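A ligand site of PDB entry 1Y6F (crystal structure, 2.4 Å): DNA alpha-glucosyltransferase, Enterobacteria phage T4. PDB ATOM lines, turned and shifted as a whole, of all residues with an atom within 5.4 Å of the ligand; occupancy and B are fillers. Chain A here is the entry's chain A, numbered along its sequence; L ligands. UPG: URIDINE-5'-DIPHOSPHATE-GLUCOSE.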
ATOM      1  N   GLY A  16      -5.416 -13.122  15.691  1.00  0.00           N
ATOM      2  CA  GLY A  16      -5.191 -12.105  14.682  1.00  0.00           C
ATOM      3  C   GLY A  16      -3.964 -11.232  14.844  1.00  0.00           C
ATOM      4  O   GLY A  16      -3.895 -10.156  14.270  1.00  0.00           O
ATOM      5  N   CYS A  17      -2.993 -11.687  15.628  1.00  0.00           N
ATOM      6  CA  CYS A  17      -1.761 -10.913  15.806  1.00  0.00           C
ATOM      7  C   CYS A  17      -0.544 -11.761  15.470  1.00  0.00           C
ATOM      8  O   CYS A  17      -0.560 -12.549  14.512  1.00  0.00           O
ATOM      9  CB  CYS A  17      -1.658 -10.370  17.237  1.00  0.00           C
ATOM     10  SG  CYS A  17      -3.034  -9.273  17.731  1.00  0.00           S
ATOM     11  N   GLY A  18       0.524 -11.607  16.244  1.00  0.00           N
ATOM     12  CA  GLY A  18       1.754 -12.361  15.996  1.00  0.00           C
ATOM     13  C   GLY A  18       1.676 -13.863  15.830  1.00  0.00           C
ATOM     14  O   GLY A  18       2.239 -14.429  14.886  1.00  0.00           O
ATOM     15  N   VAL A  19       0.987 -14.530  16.749  1.00  0.00           N
ATOM     16  CA  VAL A  19       0.855 -15.970  16.691  1.00  0.00           C
ATOM     17  C   VAL A  19       0.091 -16.411  15.438  1.00  0.00           C
ATOM     18  O   VAL A  19       0.466 -17.386  14.792  1.00  0.00           O
ATOM     19  CB  VAL A  19       0.124 -16.483  17.925  1.00  0.00           C
ATOM     20  CG1 VAL A  19      -0.172 -17.963  17.773  1.00  0.00           C
ATOM     21  CG2 VAL A  19       0.988 -16.214  19.170  1.00  0.00           C
ATOM     22  N   LYS A  21      -0.135 -14.729  12.682  1.00  0.00           N
ATOM     23  CA  LYS A  21       0.716 -14.431  11.546  1.00  0.00           C
ATOM     24  C   LYS A  21       1.822 -15.470  11.399  1.00  0.00           C
ATOM     25  O   LYS A  21       2.162 -15.865  10.290  1.00  0.00           O
ATOM     26  CB  LYS A  21       1.322 -13.037  11.702  1.00  0.00           C
ATOM     27  CG  LYS A  21       2.289 -12.630  10.603  1.00  0.00           C
ATOM     28  CD  LYS A  21       1.616 -12.630   9.240  1.00  0.00           C
ATOM     29  CE  LYS A  21       2.543 -12.023   8.187  1.00  0.00           C
ATOM     30  NZ  LYS A  21       1.921 -12.035   6.834  1.00  0.00           N
ATOM     31  N   PHE A  22       2.361 -15.938  12.515  1.00  0.00           N
ATOM     32  CA  PHE A  22       3.439 -16.925  12.440  1.00  0.00           C
ATOM     33  C   PHE A  22       2.917 -18.230  11.863  1.00  0.00           C
ATOM     34  O   PHE A  22       3.554 -18.831  11.016  1.00  0.00           O
ATOM     35  CB  PHE A  22       4.034 -17.184  13.836  1.00  0.00           C
ATOM     36  CG  PHE A  22       5.017 -18.310  13.894  1.00  0.00           C
ATOM     37  CD1 PHE A  22       6.328 -18.122  13.466  1.00  0.00           C
ATOM     38  CD2 PHE A  22       4.647 -19.549  14.409  1.00  0.00           C
ATOM     39  CE1 PHE A  22       7.266 -19.170  13.569  1.00  0.00           C
ATOM     40  CE2 PHE A  22       5.579 -20.602  14.518  1.00  0.00           C
ATOM     41  CZ  PHE A  22       6.886 -20.406  14.093  1.00  0.00           C
ATOM     42  N   ARG A  49      -9.685  -8.858  16.536  1.00  0.00           N
ATOM     43  CA  ARG A  49      -8.803  -8.879  15.370  1.00  0.00           C
ATOM     44  C   ARG A  49      -8.717 -10.217  14.642  1.00  0.00           C
ATOM     45  O   ARG A  49      -7.683 -10.548  14.081  1.00  0.00           O
ATOM     46  CB  ARG A  49      -7.415  -8.420  15.834  1.00  0.00           C
ATOM     47  CG  ARG A  49      -7.481  -7.733  17.187  1.00  0.00           C
ATOM     48  CD  ARG A  49      -6.173  -7.112  17.615  1.00  0.00           C
ATOM     49  NE  ARG A  49      -5.847  -5.920  16.850  1.00  0.00           N
ATOM     50  CZ  ARG A  49      -5.164  -4.889  17.336  1.00  0.00           C
ATOM     51  NH1 ARG A  49      -4.728  -4.901  18.587  1.00  0.00           N
ATOM     52  NH2 ARG A  49      -4.905  -3.849  16.562  1.00  0.00           N
ATOM     53  N   SER A  52      -7.907  -9.840  10.683  1.00  0.00           N
ATOM     54  CA  SER A  52      -6.748  -9.085  10.252  1.00  0.00           C
ATOM     55  C   SER A  52      -5.975  -9.771   9.135  1.00  0.00           C
ATOM     56  O   SER A  52      -5.398  -9.103   8.274  1.00  0.00           O
ATOM     57  CB  SER A  52      -5.842  -8.859  11.450  1.00  0.00           C
ATOM     58  OG  SER A  52      -6.460  -7.998  12.393  1.00  0.00           O
ATOM     59  N   HIS A  53      -5.947 -11.104   9.143  1.00  0.00           N
ATOM     60  CA  HIS A  53      -5.240 -11.855   8.103  1.00  0.00           C
ATOM     61  C   HIS A  53      -6.245 -12.752   7.382  1.00  0.00           C
ATOM     62  O   HIS A  53      -7.249 -13.136   7.969  1.00  0.00           O
ATOM     63  CB  HIS A  53      -4.148 -12.713   8.733  1.00  0.00           C
ATOM     64  CG  HIS A  53      -3.252 -11.969   9.664  1.00  0.00           C
ATOM     65  ND1 HIS A  53      -3.613 -11.669  10.957  1.00  0.00           N
ATOM     66  CD2 HIS A  53      -2.031 -11.423   9.486  1.00  0.00           C
ATOM     67  CE1 HIS A  53      -2.651 -10.972  11.544  1.00  0.00           C
ATOM     68  NE2 HIS A  53      -1.683 -10.816  10.661  1.00  0.00           N
ATOM     69  N   HIS A 117       5.494 -18.103  21.960  1.00  0.00           N
ATOM     70  CA  HIS A 117       5.597 -16.786  21.339  1.00  0.00           C
ATOM     71  C   HIS A 117       5.532 -15.564  22.242  1.00  0.00           C
ATOM     72  O   HIS A 117       5.732 -14.448  21.777  1.00  0.00           O
ATOM     73  CB  HIS A 117       4.503 -16.667  20.290  1.00  0.00           C
ATOM     74  CG  HIS A 117       4.615 -17.682  19.198  1.00  0.00           C
ATOM     75  ND1 HIS A 117       5.503 -17.554  18.149  1.00  0.00           N
ATOM     76  CD2 HIS A 117       3.965 -18.855  18.998  1.00  0.00           C
ATOM     77  CE1 HIS A 117       5.384 -18.591  17.350  1.00  0.00           C
ATOM     78  NE2 HIS A 117       4.456 -19.400  17.837  1.00  0.00           N
ATOM     79  N   HIS A 119       6.537 -13.089  25.727  1.00  0.00           N
ATOM     80  CA  HIS A 119       7.757 -12.572  26.330  1.00  0.00           C
ATOM     81  C   HIS A 119       7.734 -12.485  27.835  1.00  0.00           C
ATOM     82  O   HIS A 119       8.408 -13.231  28.527  1.00  0.00           O
ATOM     83  CB  HIS A 119       8.055 -11.187  25.774  1.00  0.00           C
ATOM     84  CG  HIS A 119       8.230 -11.152  24.287  1.00  0.00           C
ATOM     85  ND1 HIS A 119       9.262 -11.799  23.646  1.00  0.00           N
ATOM     86  CD2 HIS A 119       7.499 -10.547  23.325  1.00  0.00           C
ATOM     87  CE1 HIS A 119       9.157 -11.603  22.348  1.00  0.00           C
ATOM     88  NE2 HIS A 119       8.094 -10.851  22.123  1.00  0.00           N
ATOM     89  N   HIS A 143      11.739 -17.213  22.166  1.00  0.00           N
ATOM     90  CA  HIS A 143      12.411 -16.063  21.557  1.00  0.00           C
ATOM     91  C   HIS A 143      13.781 -15.748  22.179  1.00  0.00           C
ATOM     92  O   HIS A 143      14.580 -15.046  21.572  1.00  0.00           O
ATOM     93  CB  HIS A 143      11.542 -14.797  21.669  1.00  0.00           C
ATOM     94  CG  HIS A 143      10.407 -14.768  20.701  1.00  0.00           C
ATOM     95  ND1 HIS A 143      10.588 -14.718  19.340  1.00  0.00           N
ATOM     96  CD2 HIS A 143       9.068 -14.811  20.904  1.00  0.00           C
ATOM     97  CE1 HIS A 143       9.409 -14.748  18.744  1.00  0.00           C
ATOM     98  NE2 HIS A 143       8.475 -14.806  19.670  1.00  0.00           N
ATOM     99  N   PHE A 177      14.274 -19.352  18.177  1.00  0.00           N
ATOM    100  CA  PHE A 177      13.749 -19.253  16.825  1.00  0.00           C
ATOM    101  C   PHE A 177      13.452 -17.801  16.537  1.00  0.00           C
ATOM    102  O   PHE A 177      13.504 -16.969  17.435  1.00  0.00           O
ATOM    103  CB  PHE A 177      12.476 -20.078  16.660  1.00  0.00           C
ATOM    104  CG  PHE A 177      11.246 -19.425  17.233  1.00  0.00           C
ATOM    105  CD1 PHE A 177      10.333 -18.782  16.412  1.00  0.00           C
ATOM    106  CD2 PHE A 177      11.012 -19.451  18.612  1.00  0.00           C
ATOM    107  CE1 PHE A 177       9.187 -18.176  16.943  1.00  0.00           C
ATOM    108  CE2 PHE A 177       9.873 -18.850  19.163  1.00  0.00           C
ATOM    109  CZ  PHE A 177       8.953 -18.202  18.321  1.00  0.00           C
ATOM    110  N   PRO A 179      10.546 -15.351  14.364  1.00  0.00           N
ATOM    111  CA  PRO A 179       9.260 -15.436  13.667  1.00  0.00           C
ATOM    112  C   PRO A 179       9.491 -14.931  12.256  1.00  0.00           C
ATOM    113  O   PRO A 179       9.527 -13.727  12.017  1.00  0.00           O
ATOM    114  CB  PRO A 179       8.372 -14.524  14.508  1.00  0.00           C
ATOM    115  CG  PRO A 179       9.362 -13.477  15.006  1.00  0.00           C
ATOM    116  CD  PRO A 179      10.545 -14.301  15.397  1.00  0.00           C
ATOM    117  N   ILE A 205       2.458   1.524  13.667  1.00  0.00           N
ATOM    118  CA  ILE A 205       1.595   0.346  13.743  1.00  0.00           C
ATOM    119  C   ILE A 205       1.976  -0.458  14.980  1.00  0.00           C
ATOM    120  O   ILE A 205       3.160  -0.513  15.340  1.00  0.00           O
ATOM    121  CB  ILE A 205       1.690  -0.585  12.502  1.00  0.00           C
ATOM    122  CG1 ILE A 205       3.136  -1.066  12.311  1.00  0.00           C
ATOM    123  CG2 ILE A 205       1.157   0.136  11.268  1.00  0.00           C
ATOM    124  CD1 ILE A 205       3.337  -1.943  11.080  1.00  0.00           C
ATOM    125  N   GLY A 206       0.965  -1.052  15.602  1.00  0.00           N
ATOM    126  CA  GLY A 206       1.162  -1.855  16.800  1.00  0.00           C
ATOM    127  C   GLY A 206      -0.135  -2.124  17.551  1.00  0.00           C
ATOM    128  O   GLY A 206      -1.215  -2.209  16.954  1.00  0.00           O
ATOM    129  N   ARG A 207      -0.006  -2.277  18.865  1.00  0.00           N
ATOM    130  CA  ARG A 207      -1.152  -2.537  19.737  1.00  0.00           C
ATOM    131  C   ARG A 207      -0.971  -1.688  20.985  1.00  0.00           C
ATOM    132  O   ARG A 207       0.077  -1.083  21.188  1.00  0.00           O
ATOM    133  CB  ARG A 207      -1.181  -3.987  20.186  1.00  0.00           C
ATOM    134  CG  ARG A 207      -1.337  -5.010  19.114  1.00  0.00           C
ATOM    135  CD  ARG A 207      -1.435  -6.390  19.750  1.00  0.00           C
ATOM    136  NE  ARG A 207      -0.179  -6.869  20.343  1.00  0.00           N
ATOM    137  CZ  ARG A 207      -0.036  -7.203  21.618  1.00  0.00           C
ATOM    138  NH1 ARG A 207       1.140  -7.638  22.079  1.00  0.00           N
ATOM    139  NH2 ARG A 207      -1.062  -7.108  22.453  1.00  0.00           N
ATOM    140  N   TRP A 211       5.350  -1.646  26.074  1.00  0.00           N
ATOM    141  CA  TRP A 211       6.619  -1.901  25.399  1.00  0.00           C
ATOM    142  C   TRP A 211       6.570  -1.691  23.893  1.00  0.00           C
ATOM    143  O   TRP A 211       7.588  -1.802  23.211  1.00  0.00           O
ATOM    144  CB  TRP A 211       7.146  -3.316  25.724  1.00  0.00           C
ATOM    145  CG  TRP A 211       6.178  -4.447  25.503  1.00  0.00           C
ATOM    146  CD1 TRP A 211       5.190  -4.861  26.344  1.00  0.00           C
ATOM    147  CD2 TRP A 211       6.125  -5.315  24.358  1.00  0.00           C
ATOM    148  NE1 TRP A 211       4.524  -5.946  25.807  1.00  0.00           N
ATOM    149  CE2 TRP A 211       5.085  -6.241  24.594  1.00  0.00           C
ATOM    150  CE3 TRP A 211       6.855  -5.409  23.170  1.00  0.00           C
ATOM    151  CZ2 TRP A 211       4.753  -7.243  23.686  1.00  0.00           C
ATOM    152  CZ3 TRP A 211       6.535  -6.405  22.264  1.00  0.00           C
ATOM    153  CH2 TRP A 211       5.489  -7.310  22.530  1.00  0.00           C
ATOM    154  N   LYS A 212       5.388  -1.363  23.392  1.00  0.00           N
ATOM    155  CA  LYS A 212       5.197  -1.129  21.968  1.00  0.00           C
ATOM    156  C   LYS A 212       5.498   0.340  21.601  1.00  0.00           C
ATOM    157  O   LYS A 212       5.230   0.783  20.491  1.00  0.00           O
ATOM    158  CB  LYS A 212       3.762  -1.465  21.589  1.00  0.00           C
ATOM    159  CG  LYS A 212       3.634  -2.455  20.438  1.00  0.00           C
ATOM    160  CD  LYS A 212       4.073  -3.857  20.824  1.00  0.00           C
ATOM    161  CE  LYS A 212       4.003  -4.759  19.590  1.00  0.00           C
ATOM    162  NZ  LYS A 212       4.278  -6.196  19.870  1.00  0.00           N
ATOM    163  N   GLY A 236      -3.826   0.426  14.804  1.00  0.00           N
ATOM    164  CA  GLY A 236      -3.832  -0.738  15.661  1.00  0.00           C
ATOM    165  C   GLY A 236      -4.040  -0.538  17.145  1.00  0.00           C
ATOM    166  O   GLY A 236      -3.900  -1.482  17.914  1.00  0.00           O
ATOM    167  N   CYS A 277      -8.195  -0.966  14.780  1.00  0.00           N
ATOM    168  CA  CYS A 277      -7.507  -2.217  14.504  1.00  0.00           C
ATOM    169  C   CYS A 277      -7.475  -2.271  12.989  1.00  0.00           C
ATOM    170  O   CYS A 277      -8.232  -1.559  12.332  1.00  0.00           O
ATOM    171  CB  CYS A 277      -8.289  -3.420  15.067  1.00  0.00           C
ATOM    172  SG  CYS A 277      -9.531  -4.111  13.954  1.00  0.00           S
ATOM    173  N   TYR A 278      -6.639  -3.103  12.397  1.00  0.00           N
ATOM    174  CA  TYR A 278      -6.580  -3.089  10.959  1.00  0.00           C
ATOM    175  C   TYR A 278      -6.495  -4.425  10.284  1.00  0.00           C
ATOM    176  O   TYR A 278      -6.183  -5.437  10.910  1.00  0.00           O
ATOM    177  CB  TYR A 278      -5.404  -2.227  10.492  1.00  0.00           C
ATOM    178  CG  TYR A 278      -4.045  -2.728  10.945  1.00  0.00           C
ATOM    179  CD1 TYR A 278      -3.349  -3.705  10.221  1.00  0.00           C
ATOM    180  CD2 TYR A 278      -3.432  -2.217  12.085  1.00  0.00           C
ATOM    181  CE1 TYR A 278      -2.089  -4.131  10.622  1.00  0.00           C
ATOM    182  CE2 TYR A 278      -2.183  -2.641  12.495  1.00  0.00           C
ATOM    183  CZ  TYR A 278      -1.509  -3.602  11.762  1.00  0.00           C
ATOM    184  OH  TYR A 278      -0.257  -3.993  12.154  1.00  0.00           O
ATOM    185  N   ILE A 279      -6.772  -4.382   8.987  1.00  0.00           N
ATOM    186  CA  ILE A 279      -6.695  -5.551   8.149  1.00  0.00           C
ATOM    187  C   ILE A 279      -5.276  -5.423   7.620  1.00  0.00           C
ATOM    188  O   ILE A 279      -4.907  -4.412   7.043  1.00  0.00           O
ATOM    189  CB  ILE A 279      -7.719  -5.470   7.015  1.00  0.00           C
ATOM    190  CG1 ILE A 279      -9.120  -5.639   7.612  1.00  0.00           C
ATOM    191  CG2 ILE A 279      -7.452  -6.544   5.980  1.00  0.00           C
ATOM    192  CD1 ILE A 279     -10.194  -5.896   6.572  1.00  0.00           C
ATOM    193  N   ASN A 280      -4.477  -6.457   7.868  1.00  0.00           N
ATOM    194  CA  ASN A 280      -3.082  -6.454   7.474  1.00  0.00           C
ATOM    195  C   ASN A 280      -2.756  -6.054   6.029  1.00  0.00           C
ATOM    196  O   ASN A 280      -1.875  -5.234   5.818  1.00  0.00           O
ATOM    197  CB  ASN A 280      -2.480  -7.828   7.797  1.00  0.00           C
ATOM    198  CG  ASN A 280      -0.980  -7.843   7.658  1.00  0.00           C
ATOM    199  OD1 ASN A 280      -0.447  -8.124   6.586  1.00  0.00           O
ATOM    200  ND2 ASN A 280      -0.287  -7.532   8.743  1.00  0.00           N
ATOM    201  N   MET A 283      -3.383  -2.307   5.617  1.00  0.00           N
ATOM    202  CA  MET A 283      -2.342  -1.524   6.250  1.00  0.00           C
ATOM    203  C   MET A 283      -1.085  -1.450   5.388  1.00  0.00           C
ATOM    204  O   MET A 283      -0.560  -0.364   5.174  1.00  0.00           O
ATOM    205  CB  MET A 283      -2.014  -2.114   7.636  1.00  0.00           C
ATOM    206  CG  MET A 283      -0.906  -1.396   8.400  1.00  0.00           C
ATOM    207  SD  MET A 283       0.741  -1.841   7.810  1.00  0.00           S
ATOM    208  CE  MET A 283       0.990  -3.353   8.711  1.00  0.00           C
ATOM    209  N   GLN A 295       7.801   1.710  14.436  1.00  0.00           N
ATOM    210  CA  GLN A 295       7.582   0.485  15.216  1.00  0.00           C
ATOM    211  C   GLN A 295       8.555   0.622  16.364  1.00  0.00           C
ATOM    212  O   GLN A 295       9.699   0.176  16.286  1.00  0.00           O
ATOM    213  CB  GLN A 295       7.902  -0.738  14.358  1.00  0.00           C
ATOM    214  CG  GLN A 295       7.121  -1.997  14.726  1.00  0.00           C
ATOM    215  CD  GLN A 295       7.730  -2.755  15.883  1.00  0.00           C
ATOM    216  OE1 GLN A 295       8.469  -2.189  16.684  1.00  0.00           O
ATOM    217  NE2 GLN A 295       7.416  -4.030  15.982  1.00  0.00           N
ATOM    218  N   LEU A 299      11.317  -3.564  23.979  1.00  0.00           N
ATOM    219  CA  LEU A 299      11.426  -4.735  24.830  1.00  0.00           C
ATOM    220  C   LEU A 299      12.760  -4.687  25.595  1.00  0.00           C
ATOM    221  O   LEU A 299      13.656  -3.932  25.232  1.00  0.00           O
ATOM    222  CB  LEU A 299      11.379  -5.977  23.945  1.00  0.00           C
ATOM    223  CG  LEU A 299      10.589  -7.224  24.333  1.00  0.00           C
ATOM    224  CD1 LEU A 299       9.172  -6.843  24.758  1.00  0.00           C
ATOM    225  CD2 LEU A 299      10.568  -8.171  23.127  1.00  0.00           C
ATOM    226  N   LEU A 308      12.973 -10.194  15.569  1.00  0.00           N
ATOM    227  CA  LEU A 308      12.399  -8.927  15.190  1.00  0.00           C
ATOM    228  C   LEU A 308      10.901  -9.325  15.160  1.00  0.00           C
ATOM    229  O   LEU A 308      10.582 -10.522  15.206  1.00  0.00           O
ATOM    230  CB  LEU A 308      12.920  -8.539  13.802  1.00  0.00           C
ATOM    231  CG  LEU A 308      13.315  -7.090  13.554  1.00  0.00           C
ATOM    232  CD1 LEU A 308      14.034  -6.528  14.770  1.00  0.00           C
ATOM    233  CD2 LEU A 308      14.199  -7.009  12.313  1.00  0.00           C
ATOM    234  N   GLU A 309       9.987  -8.367  15.136  1.00  0.00           N
ATOM    235  CA  GLU A 309       8.555  -8.658  15.106  1.00  0.00           C
ATOM    236  C   GLU A 309       7.976  -8.496  13.704  1.00  0.00           C
ATOM    237  O   GLU A 309       8.572  -7.825  12.864  1.00  0.00           O
ATOM    238  CB  GLU A 309       7.814  -7.722  16.058  1.00  0.00           C
ATOM    239  CG  GLU A 309       7.894  -8.148  17.513  1.00  0.00           C
ATOM    240  CD  GLU A 309       7.643  -7.006  18.489  1.00  0.00           C
ATOM    241  OE1 GLU A 309       8.621  -6.345  18.882  1.00  0.00           O
ATOM    242  OE2 GLU A 309       6.470  -6.768  18.846  1.00  0.00           O
ATOM    243  N   TYR A 310       6.822  -9.107  13.433  1.00  0.00           N
ATOM    244  CA  TYR A 310       6.239  -8.976  12.102  1.00  0.00           C
ATOM    245  C   TYR A 310       6.019  -7.527  11.682  1.00  0.00           C
ATOM    246  O   TYR A 310       6.206  -7.185  10.506  1.00  0.00           O
ATOM    247  CB  TYR A 310       4.925  -9.749  11.995  1.00  0.00           C
ATOM    248  CG  TYR A 310       5.171 -11.226  11.905  1.00  0.00           C
ATOM    249  CD1 TYR A 310       4.909 -12.074  12.985  1.00  0.00           C
ATOM    250  CD2 TYR A 310       5.746 -11.770  10.764  1.00  0.00           C
ATOM    251  CE1 TYR A 310       5.229 -13.421  12.941  1.00  0.00           C
ATOM    252  CE2 TYR A 310       6.065 -13.107  10.694  1.00  0.00           C
ATOM    253  CZ  TYR A 310       5.807 -13.932  11.783  1.00  0.00           C
ATOM    254  OH  TYR A 310       6.143 -15.262  11.685  1.00  0.00           O
ATOM    255  N   THR A 311       5.623  -6.669  12.633  1.00  0.00           N
ATOM    256  CA  THR A 311       5.423  -5.257  12.305  1.00  0.00           C
ATOM    257  C   THR A 311       6.764  -4.659  11.848  1.00  0.00           C
ATOM    258  O   THR A 311       6.770  -3.766  11.011  1.00  0.00           O
ATOM    259  CB  THR A 311       4.843  -4.436  13.496  1.00  0.00           C
ATOM    260  OG1 THR A 311       5.315  -4.953  14.739  1.00  0.00           O
ATOM    261  CG2 THR A 311       3.326  -4.503  13.484  1.00  0.00           C
ATOM    262  N   HIS A 312       7.885  -5.153  12.386  1.00  0.00           N
ATOM    263  CA  HIS A 312       9.203  -4.672  11.984  1.00  0.00           C
ATOM    264  C   HIS A 312       9.398  -5.063  10.512  1.00  0.00           C
ATOM    265  O   HIS A 312       9.700  -4.222   9.662  1.00  0.00           O
ATOM    266  CB  HIS A 312      10.345  -5.340  12.782  1.00  0.00           C
ATOM    267  CG  HIS A 312      10.477  -4.874  14.206  1.00  0.00           C
ATOM    268  ND1 HIS A 312      10.888  -3.606  14.538  1.00  0.00           N
ATOM    269  CD2 HIS A 312      10.283  -5.527  15.372  1.00  0.00           C
ATOM    270  CE1 HIS A 312      10.953  -3.497  15.861  1.00  0.00           C
ATOM    271  NE2 HIS A 312      10.596  -4.649  16.385  1.00  0.00           N
ATOM    272  N   GLU A 314       7.236  -5.982   8.185  1.00  0.00           N
ATOM    273  CA  GLU A 314       6.302  -5.443   7.205  1.00  0.00           C
ATOM    274  C   GLU A 314       6.755  -4.068   6.701  1.00  0.00           C
ATOM    275  O   GLU A 314       6.614  -3.763   5.505  1.00  0.00           O
ATOM    276  CB  GLU A 314       4.896  -5.387   7.802  1.00  0.00           C
ATOM    277  CG  GLU A 314       4.209  -6.753   7.833  1.00  0.00           C
ATOM    278  CD  GLU A 314       3.140  -6.856   8.905  1.00  0.00           C
ATOM    279  OE1 GLU A 314       2.360  -7.835   8.894  1.00  0.00           O
ATOM    280  OE2 GLU A 314       3.070  -5.958   9.770  1.00  0.00           O
HETATM  281  N1  UPG L   1      -1.834  -6.820  12.768  1.00  0.00           N
HETATM  282  C2  UPG L   1      -2.942  -6.685  11.967  1.00  0.00           C
HETATM  283  N3  UPG L   1      -3.951  -5.940  12.515  1.00  0.00           N
HETATM  284  C4  UPG L   1      -3.959  -5.318  13.744  1.00  0.00           C
HETATM  285  C5  UPG L   1      -2.760  -5.480  14.495  1.00  0.00           C
HETATM  286  C6  UPG L   1      -1.757  -6.209  13.990  1.00  0.00           C
HETATM  287  O2  UPG L   1      -3.025  -7.188  10.860  1.00  0.00           O
HETATM  288  O4  UPG L   1      -4.974  -4.740  14.125  1.00  0.00           O
HETATM  289  C1C UPG L   1      -0.742  -7.673  12.275  1.00  0.00           C
HETATM  290  C2C UPG L   1       0.613  -6.992  12.090  1.00  0.00           C
HETATM  291  O2C UPG L   1       0.687  -6.426  10.796  1.00  0.00           O
HETATM  292  C3C UPG L   1       1.553  -8.191  12.242  1.00  0.00           C
HETATM  293  C4C UPG L   1       0.880  -8.985  13.355  1.00  0.00           C
HETATM  294  O4C UPG L   1      -0.542  -8.675  13.247  1.00  0.00           O
HETATM  295  O3C UPG L   1       1.562  -8.958  11.050  1.00  0.00           O
HETATM  296  C5C UPG L   1       1.352  -8.672  14.749  1.00  0.00           C
HETATM  297  O5C UPG L   1       2.593  -9.321  14.985  1.00  0.00           O
HETATM  298  PA  UPG L   1       3.782  -8.615  15.772  1.00  0.00           P
HETATM  299  O1A UPG L   1       4.793  -9.672  15.999  1.00  0.00           O
HETATM  300  O2A UPG L   1       4.168  -7.389  15.034  1.00  0.00           O
HETATM  301  O3A UPG L   1       3.112  -8.156  17.186  1.00  0.00           O
HETATM  302  PB  UPG L   1       2.448  -9.029  18.389  1.00  0.00           P
HETATM  303  O1B UPG L   1       2.931  -8.472  19.663  1.00  0.00           O
HETATM  304  O2B UPG L   1       1.001  -9.078  18.118  1.00  0.00           O
HETATM  305  O3B UPG L   1       3.091 -10.487  18.182  1.00  0.00           O
HETATM  306  C1' UPG L   1       3.468 -11.438  19.236  1.00  0.00           C
HETATM  307  C2' UPG L   1       4.639 -11.004  20.111  1.00  0.00           C
HETATM  308  C3' UPG L   1       5.828 -10.701  19.186  1.00  0.00           C
HETATM  309  C4' UPG L   1       6.181 -11.957  18.368  1.00  0.00           C
HETATM  310  C5' UPG L   1       4.949 -12.549  17.661  1.00  0.00           C
HETATM  311  C6' UPG L   1       5.199 -13.926  17.072  1.00  0.00           C
HETATM  312  O2' UPG L   1       4.301  -9.885  20.901  1.00  0.00           O
HETATM  313  O3' UPG L   1       6.951 -10.255  19.932  1.00  0.00           O
HETATM  314  O4' UPG L   1       7.155 -11.617  17.387  1.00  0.00           O
HETATM  315  O5' UPG L   1       3.819 -12.678  18.589  1.00  0.00           O
HETATM  316  O6' UPG L   1       6.372 -14.532  17.628  1.00  0.00           O
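O2 of the ligand sits close to N of Asn 280, at 3.4 Å. The side-chain amide nitrogen (ND2) of Asn 280 sits at hydrogen-bond distance from an oxygen (O2C) of the ligand (2.5 Å). O3' of the ligand lies within hydrogen-bond range of NE2 of His 119 (2.5 Å). An oxygen (O3C) of the ligand is in hydrogen-bond range of the side-chain carboxylate (OE1) of Glu 314 (2.6 Å). O4 of the ligand is in hydrogen-bond range of NH2 of Arg 49 (2.6 Å). An oxygen (O1B) of the ligand is in salt-bridge range of the side-chain amino group (NZ) of Lys 212. N of Thr 311 sits at hydrogen-bond distance from O2A of the ligand (2.9 Å). An oxygen (O2A) of the ligand lies within hydrogen-bond range of the side-chain hydroxyl (OG1) of Thr 311 (2.7 Å). N of Tyr 278 lies within hydrogen-bond range of O4 of the ligand, 2.9 Å away. O of Tyr 278 lies within hydrogen-bond range of N3 of the ligand (2.8 Å). The side-chain hydroxyl of Tyr 278 is in hydrogen-bond range of an oxygen (O2C) of the ligand, 2.9 Å away. A ring nitrogen (NE2) of His 143 sits at hydrogen-bond distance from an oxygen (O6') of the ligand (2.9 Å). NH1 of Arg 207 lies within salt-bridge range of O1B of the ligand, 3.1 Å away. The backbone NH (N) of Gly 18 lies within hydrogen-bond range of an oxygen (O2B) of the ligand, 3.2 Å away. An oxygen (O6') of the ligand sits at hydrogen-bond distance from a ring nitrogen (ND1) of His 117. N3 of the ligand sits at hydrogen-bond distance from OG of Ser 52 (3.2 Å). N of Tyr 310 lies within hydrogen-bond range of O1A of the ligand, 3.3 Å away.
ND2 of Asn 280 lies within hydrogen-bond range of OE1 of Glu 314 (2.7 Å). The backbone NH of Asn 280 is in hydrogen-bond range of the backbone carbonyl oxygen of Ser 52. The backbone carbonyl oxygen (O) of Arg 49 is in hydrogen-bond range of the side-chain hydroxyl (OG) of Ser 52 (3.3 Å). The guanidinium group of Arg 49 lies within hydrogen-bond range of the backbone carbonyl oxygen of Gly 236 (2.9 Å). NZ of Lys 212 is in salt-bridge range of OE2 of Glu 309, at 2.5 Å. OG1 of Thr 311 sits at hydrogen-bond distance from NE2 of Gln 295, at 2.6 Å. The side-chain hydroxyl (OG) of Ser 52 is in hydrogen-bond range of the backbone carbonyl oxygen (O) of Tyr 278 (3.0 Å). A ring nitrogen (NE2) of His 143 lies close to the backbone carbonyl oxygen (O) of His 117.
O of Gly 16 touches O4C of the ligand, at 3.8 Å. CB of Cys 17 touches O2B of the ligand, 3.1 Å away. Val 19 touches the ligand (N to O5', 3.9 Å). Lys 21 touches the ligand. NE2 of His 53 touches O4C of the ligand, 3.5 Å away. Pro 179 touches the ligand. CH2 of Trp 211 touches O2' of the ligand (3.3 Å). CA of Cys 277 touches O4 of the ligand, at 3.6 Å. Met 283 touches the ligand. Glu 309 touches the ligand. Hydrophobic or aromatic side chains that line the ligand: His 53, His 117, His 119, His 143, Pro 179, Trp 211, Tyr 278, Met 283 and Tyr 310. Within 4 Å of the ligand: Gly 16, Cys 17, Gly 18, Val 19, Lys 21, Arg 49, Ser 52, His 53, His 117, His 119, His 143, Pro 179, Arg 207, Trp 211, Lys 212, Cys 277, Tyr 278, Asn 280, Met 283, Glu 309, Tyr 310, Thr 311 and Glu 314.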
